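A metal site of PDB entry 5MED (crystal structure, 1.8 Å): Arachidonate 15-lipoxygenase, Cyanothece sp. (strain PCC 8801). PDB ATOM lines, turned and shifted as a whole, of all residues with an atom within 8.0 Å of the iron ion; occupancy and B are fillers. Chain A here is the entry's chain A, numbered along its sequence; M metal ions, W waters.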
ATOM      1  N   HIS A 252      -9.297   2.162  15.410  1.00  0.00           N
ATOM      2  CA  HIS A 252     -10.468   1.530  15.979  1.00  0.00           C
ATOM      3  C   HIS A 252     -11.722   2.359  15.758  1.00  0.00           C
ATOM      4  O   HIS A 252     -12.719   1.873  15.190  1.00  0.00           O
ATOM      5  CB  HIS A 252     -10.293   1.240  17.459  1.00  0.00           C
ATOM      6  CG  HIS A 252     -11.546   0.770  18.126  1.00  0.00           C
ATOM      7  ND1 HIS A 252     -12.467   1.641  18.667  1.00  0.00           N
ATOM      8  CD2 HIS A 252     -12.066  -0.466  18.272  1.00  0.00           C
ATOM      9  CE1 HIS A 252     -13.485   0.943  19.146  1.00  0.00           C
ATOM     10  NE2 HIS A 252     -13.261  -0.338  18.926  1.00  0.00           N
ATOM     11  N   GLU A 253     -11.714   3.586  16.264  1.00  0.00           N
ATOM     12  CA  GLU A 253     -12.975   4.336  16.260  1.00  0.00           C
ATOM     13  C   GLU A 253     -13.390   4.720  14.861  1.00  0.00           C
ATOM     14  O   GLU A 253     -14.571   4.609  14.510  1.00  0.00           O
ATOM     15  CB  GLU A 253     -12.883   5.568  17.150  1.00  0.00           C
ATOM     16  CG  GLU A 253     -12.828   5.251  18.640  1.00  0.00           C
ATOM     17  CD  GLU A 253     -14.016   4.431  19.162  1.00  0.00           C
ATOM     18  OE1 GLU A 253     -14.993   4.169  18.427  1.00  0.00           O
ATOM     19  OE2 GLU A 253     -13.943   4.025  20.350  1.00  0.00           O
ATOM     20  N   HIS A 257     -14.867   0.557  14.008  1.00  0.00           N
ATOM     21  CA  HIS A 257     -16.153   0.723  14.687  1.00  0.00           C
ATOM     22  C   HIS A 257     -17.119   1.596  13.883  1.00  0.00           C
ATOM     23  O   HIS A 257     -18.129   1.085  13.415  1.00  0.00           O
ATOM     24  CB  HIS A 257     -15.881   1.265  16.093  1.00  0.00           C
ATOM     25  CG  HIS A 257     -17.097   1.364  16.955  1.00  0.00           C
ATOM     26  ND1 HIS A 257     -17.196   2.264  17.995  1.00  0.00           N
ATOM     27  CD2 HIS A 257     -18.285   0.735  16.892  1.00  0.00           C
ATOM     28  CE1 HIS A 257     -18.385   2.159  18.545  1.00  0.00           C
ATOM     29  NE2 HIS A 257     -19.068   1.242  17.897  1.00  0.00           N
ATOM     30  N   LEU A 258     -16.848   2.891  13.724  1.00  0.00           N
ATOM     31  CA  LEU A 258     -17.807   3.747  13.039  1.00  0.00           C
ATOM     32  C   LEU A 258     -18.003   3.337  11.590  1.00  0.00           C
ATOM     33  O   LEU A 258     -19.137   3.098  11.150  1.00  0.00           O
ATOM     34  CB  LEU A 258     -17.362   5.202  13.119  1.00  0.00           C
ATOM     35  CG  LEU A 258     -17.847   5.947  14.357  1.00  0.00           C
ATOM     36  CD1 LEU A 258     -17.238   7.347  14.408  1.00  0.00           C
ATOM     37  CD2 LEU A 258     -19.386   5.992  14.323  1.00  0.00           C
ATOM     38  N   THR A 261     -18.826  -1.033  11.047  1.00  0.00           N
ATOM     39  CA  THR A 261     -20.032  -1.661  11.542  1.00  0.00           C
ATOM     40  C   THR A 261     -21.203  -0.696  11.301  1.00  0.00           C
ATOM     41  O   THR A 261     -21.903  -0.827  10.299  1.00  0.00           O
ATOM     42  CB  THR A 261     -19.898  -2.123  13.004  1.00  0.00           C
ATOM     43  OG1 THR A 261     -19.628  -1.003  13.866  1.00  0.00           O
ATOM     44  CG2 THR A 261     -18.737  -3.153  13.125  1.00  0.00           C
ATOM     45  N   HIS A 262     -21.338   0.342  12.153  1.00  0.00           N
ATOM     46  CA  HIS A 262     -22.404   1.325  12.030  1.00  0.00           C
ATOM     47  C   HIS A 262     -22.693   1.802  10.595  1.00  0.00           C
ATOM     48  O   HIS A 262     -23.827   1.659  10.111  1.00  0.00           O
ATOM     49  CB  HIS A 262     -22.052   2.516  12.912  1.00  0.00           C
ATOM     50  CG  HIS A 262     -22.197   2.257  14.372  1.00  0.00           C
ATOM     51  ND1 HIS A 262     -23.396   2.409  15.030  1.00  0.00           N
ATOM     52  CD2 HIS A 262     -21.326   1.788  15.295  1.00  0.00           C
ATOM     53  CE1 HIS A 262     -23.253   2.085  16.301  1.00  0.00           C
ATOM     54  NE2 HIS A 262     -22.004   1.704  16.483  1.00  0.00           N
ATOM     55  N   ILE A 296     -29.338   4.638  16.175  1.00  0.00           N
ATOM     56  CA  ILE A 296     -28.014   4.823  16.774  1.00  0.00           C
ATOM     57  C   ILE A 296     -27.104   5.554  15.799  1.00  0.00           C
ATOM     58  O   ILE A 296     -26.259   6.364  16.196  1.00  0.00           O
ATOM     59  CB  ILE A 296     -27.404   3.493  17.291  1.00  0.00           C
ATOM     60  CG1 ILE A 296     -26.200   3.740  18.213  1.00  0.00           C
ATOM     61  CG2 ILE A 296     -26.964   2.554  16.146  1.00  0.00           C
ATOM     62  CD1 ILE A 296     -26.544   4.499  19.512  1.00  0.00           C
ATOM     63  N   ASN A 297     -27.303   5.338  14.479  1.00  0.00           N
ATOM     64  CA  ASN A 297     -26.533   6.093  13.492  1.00  0.00           C
ATOM     65  C   ASN A 297     -26.946   7.561  13.426  1.00  0.00           C
ATOM     66  O   ASN A 297     -26.099   8.428  13.147  1.00  0.00           O
ATOM     67  CB  ASN A 297     -26.632   5.442  12.115  1.00  0.00           C
ATOM     68  CG  ASN A 297     -25.795   4.176  12.017  1.00  0.00           C
ATOM     69  OD1 ASN A 297     -24.982   3.927  12.901  1.00  0.00           O
ATOM     70  ND2 ASN A 297     -26.014   3.373  10.988  1.00  0.00           N
ATOM     71  N   LEU A 304     -21.458  12.160  17.704  1.00  0.00           N
ATOM     72  CA  LEU A 304     -20.135  11.597  17.460  1.00  0.00           C
ATOM     73  C   LEU A 304     -19.362  12.298  16.353  1.00  0.00           C
ATOM     74  O   LEU A 304     -18.189  12.613  16.533  1.00  0.00           O
ATOM     75  CB  LEU A 304     -20.248  10.122  17.125  1.00  0.00           C
ATOM     76  CG  LEU A 304     -20.085   9.135  18.280  1.00  0.00           C
ATOM     77  CD1 LEU A 304     -20.385   7.780  17.774  1.00  0.00           C
ATOM     78  CD2 LEU A 304     -18.652   9.179  18.741  1.00  0.00           C
ATOM     79  N   HIS A 449     -19.895  -6.052  15.465  1.00  0.00           N
ATOM     80  CA  HIS A 449     -20.079  -4.864  16.279  1.00  0.00           C
ATOM     81  C   HIS A 449     -19.854  -5.162  17.764  1.00  0.00           C
ATOM     82  O   HIS A 449     -19.259  -4.365  18.474  1.00  0.00           O
ATOM     83  CB  HIS A 449     -21.446  -4.266  16.036  1.00  0.00           C
ATOM     84  CG  HIS A 449     -21.702  -3.091  16.899  1.00  0.00           C
ATOM     85  ND1 HIS A 449     -22.509  -3.141  18.002  1.00  0.00           N
ATOM     86  CD2 HIS A 449     -21.161  -1.847  16.889  1.00  0.00           C
ATOM     87  CE1 HIS A 449     -22.504  -1.971  18.614  1.00  0.00           C
ATOM     88  NE2 HIS A 449     -21.696  -1.168  17.952  1.00  0.00           N
ATOM     89  N   ALA A 450     -20.281  -6.345  18.241  1.00  0.00           N
ATOM     90  CA  ALA A 450     -19.983  -6.690  19.639  1.00  0.00           C
ATOM     91  C   ALA A 450     -18.486  -6.750  19.897  1.00  0.00           C
ATOM     92  O   ALA A 450     -17.993  -6.216  20.911  1.00  0.00           O
ATOM     93  CB  ALA A 450     -20.653  -8.009  20.004  1.00  0.00           C
ATOM     94  N   VAL A 452     -16.012  -5.151  18.435  1.00  0.00           N
ATOM     95  CA  VAL A 452     -15.293  -3.869  18.457  1.00  0.00           C
ATOM     96  C   VAL A 452     -15.918  -2.855  19.406  1.00  0.00           C
ATOM     97  O   VAL A 452     -15.238  -1.909  19.817  1.00  0.00           O
ATOM     98  CB  VAL A 452     -15.150  -3.252  17.040  1.00  0.00           C
ATOM     99  CG1 VAL A 452     -14.408  -4.223  16.108  1.00  0.00           C
ATOM    100  CG2 VAL A 452     -16.509  -2.815  16.484  1.00  0.00           C
ATOM    101  N   ASN A 453     -17.185  -3.040  19.784  1.00  0.00           N
ATOM    102  CA  ASN A 453     -17.848  -2.081  20.648  1.00  0.00           C
ATOM    103  C   ASN A 453     -17.650  -2.400  22.129  1.00  0.00           C
ATOM    104  O   ASN A 453     -17.251  -1.516  22.909  1.00  0.00           O
ATOM    105  CB  ASN A 453     -19.342  -2.007  20.316  1.00  0.00           C
ATOM    106  CG  ASN A 453     -20.085  -0.933  21.094  1.00  0.00           C
ATOM    107  OD1 ASN A 453     -20.277   0.178  20.570  1.00  0.00           O
ATOM    108  ND2 ASN A 453     -20.559  -1.241  22.297  1.00  0.00           N
ATOM    109  N   TYR A 454     -17.878  -3.634  22.526  1.00  0.00           N
ATOM    110  CA  TYR A 454     -17.899  -3.859  23.969  1.00  0.00           C
ATOM    111  C   TYR A 454     -16.546  -3.922  24.682  1.00  0.00           C
ATOM    112  O   TYR A 454     -16.517  -3.710  25.903  1.00  0.00           O
ATOM    113  CB  TYR A 454     -18.754  -5.080  24.289  1.00  0.00           C
ATOM    114  CG  TYR A 454     -20.212  -4.727  24.169  1.00  0.00           C
ATOM    115  CD1 TYR A 454     -20.857  -3.997  25.173  1.00  0.00           C
ATOM    116  CD2 TYR A 454     -20.967  -5.056  23.047  1.00  0.00           C
ATOM    117  CE1 TYR A 454     -22.201  -3.644  25.072  1.00  0.00           C
ATOM    118  CE2 TYR A 454     -22.314  -4.695  22.923  1.00  0.00           C
ATOM    119  CZ  TYR A 454     -22.929  -3.990  23.951  1.00  0.00           C
ATOM    120  OH  TYR A 454     -24.247  -3.623  23.848  1.00  0.00           O
ATOM    121  N   GLN A 456     -14.504  -1.565  24.440  1.00  0.00           N
ATOM    122  CA  GLN A 456     -14.084  -0.169  24.542  1.00  0.00           C
ATOM    123  C   GLN A 456     -13.870   0.228  25.989  1.00  0.00           C
ATOM    124  O   GLN A 456     -12.939   0.965  26.295  1.00  0.00           O
ATOM    125  CB  GLN A 456     -15.109   0.731  23.874  1.00  0.00           C
ATOM    126  CG  GLN A 456     -15.021   0.741  22.363  1.00  0.00           C
ATOM    127  CD  GLN A 456     -16.195   1.445  21.727  1.00  0.00           C
ATOM    128  OE1 GLN A 456     -17.338   1.077  21.938  1.00  0.00           O
ATOM    129  NE2 GLN A 456     -15.908   2.516  20.985  1.00  0.00           N
ATOM    130  N   LEU A 506     -21.126   3.784  25.583  1.00  0.00           N
ATOM    131  CA  LEU A 506     -21.182   2.808  24.505  1.00  0.00           C
ATOM    132  C   LEU A 506     -21.224   1.372  25.015  1.00  0.00           C
ATOM    133  O   LEU A 506     -21.577   0.465  24.240  1.00  0.00           O
ATOM    134  CB  LEU A 506     -19.997   2.987  23.569  1.00  0.00           C
ATOM    135  CG  LEU A 506     -19.809   4.336  22.890  1.00  0.00           C
ATOM    136  CD1 LEU A 506     -18.609   4.287  21.947  1.00  0.00           C
ATOM    137  CD2 LEU A 506     -21.073   4.772  22.138  1.00  0.00           C
ATOM    138  N   CYS A 507     -20.933   1.140  26.292  1.00  0.00           N
ATOM    139  CA  CYS A 507     -20.824  -0.219  26.780  1.00  0.00           C
ATOM    140  C   CYS A 507     -21.808  -0.567  27.894  1.00  0.00           C
ATOM    141  O   CYS A 507     -21.752  -1.693  28.416  1.00  0.00           O
ATOM    142  CB  CYS A 507     -19.408  -0.489  27.284  1.00  0.00           C
ATOM    143  SG  CYS A 507     -18.203  -0.400  25.959  1.00  0.00           S
ATOM    144  N   SER A 566     -28.323  -6.710  16.930  1.00  0.00           N
ATOM    145  CA  SER A 566     -28.170  -5.656  15.938  1.00  0.00           C
ATOM    146  C   SER A 566     -27.152  -4.634  16.431  1.00  0.00           C
ATOM    147  O   SER A 566     -26.882  -4.532  17.632  1.00  0.00           O
ATOM    148  CB  SER A 566     -29.500  -4.966  15.667  1.00  0.00           C
ATOM    149  OG  SER A 566     -29.896  -4.206  16.794  1.00  0.00           O
ATOM    150  N   THR A 567     -26.607  -3.857  15.498  1.00  0.00           N
ATOM    151  CA  THR A 567     -25.796  -2.730  15.882  1.00  0.00           C
ATOM    152  C   THR A 567     -26.704  -1.625  16.421  1.00  0.00           C
ATOM    153  O   THR A 567     -27.494  -1.041  15.660  1.00  0.00           O
ATOM    154  CB  THR A 567     -24.949  -2.262  14.696  1.00  0.00           C
ATOM    155  OG1 THR A 567     -23.971  -3.270  14.428  1.00  0.00           O
ATOM    156  CG2 THR A 567     -24.224  -0.973  15.032  1.00  0.00           C
ATOM    157  N   SER A 568     -26.607  -1.346  17.711  1.00  0.00           N
ATOM    158  CA  SER A 568     -27.688  -0.608  18.364  1.00  0.00           C
ATOM    159  C   SER A 568     -27.150   0.262  19.499  1.00  0.00           C
ATOM    160  O   SER A 568     -27.960   0.874  20.204  1.00  0.00           O
ATOM    161  CB  SER A 568     -28.753  -1.565  18.904  1.00  0.00           C
ATOM    162  OG  SER A 568     -28.149  -2.662  19.568  1.00  0.00           O
ATOM    163  N   ILE A 569     -25.837   0.366  19.671  1.00  0.00           N
ATOM    164  CA  ILE A 569     -25.269   1.167  20.731  1.00  0.00           C
ATOM    165  C   ILE A 569     -23.883   1.617  20.236  1.00  0.00           C
ATOM    166  O   ILE A 569     -23.355   1.014  19.296  1.00  0.00           O
ATOM    167  CB  ILE A 569     -25.230   0.385  22.074  1.00  0.00           C
ATOM    168  CG1 ILE A 569     -24.872   1.292  23.243  1.00  0.00           C
ATOM    169  CG2 ILE A 569     -24.234  -0.814  21.994  1.00  0.00           C
ATOM    170  CD1 ILE A 569     -25.079   0.629  24.598  1.00  0.00           C
ATOM    171  OXT ILE A 569     -23.299   2.588  20.747  1.00  0.00           O
HETATM  172 FE    FE M   1     -21.256   0.908  18.410  1.00  0.00          FE
HETATM  173  O   HOH W   1     -21.138   2.793  19.318  1.00  0.00           O
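The backbone carbonyl oxygen (O) of Asn 453 lies within hydrogen-bond range of the side-chain sulfur (SG) of Cys 507, 3.4 Å away. The backbone carbonyl oxygen (O) of His 262 is in hydrogen-bond range of the side-chain amide nitrogen (ND2) of Asn 297. A ring nitrogen (ND1) of His 257 lies within hydrogen-bond range of the side-chain amide nitrogen (NE2) of Gln 456 (3.3 Å). The backbone NH of His 257 lies within hydrogen-bond range of the backbone carbonyl oxygen of His 252 (2.8 Å). The backbone carbonyl oxygen (O) of Leu 506 is in hydrogen-bond range of the side-chain amide nitrogen (ND2) of Asn 453, 2.8 Å away. The side-chain hydroxyl of Thr 261 is in hydrogen-bond range of the backbone carbonyl oxygen of His 257, at 2.6 Å. O of Asn 453 lies close to OE1 of Gln 456 (2.8 Å). A ring nitrogen (ND1) of His 257 sits at hydrogen-bond distance from the side-chain carboxylate (OE1) of Glu 253.
Within 4 Å of the iron ion: His 257, His 262, His 449, Asn 453 and Ile 569. The nearest printed residue that does not touch the iron ion is Thr 567 (4.9 Å).
The iron ion is bound by water W1 (2.1 Å), a ring nitrogen (NE2) of His 449 (2.2 Å), a ring nitrogen (NE2) of His 262 (2.2 Å), a ring nitrogen (NE2) of His 257 (2.3 Å), the chain-end carboxylate of Ile 569 (2.3 Å) and the side-chain amide oxygen of Asn 453 (2.5 Å). The iron ion has six donor atoms within binding distance.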
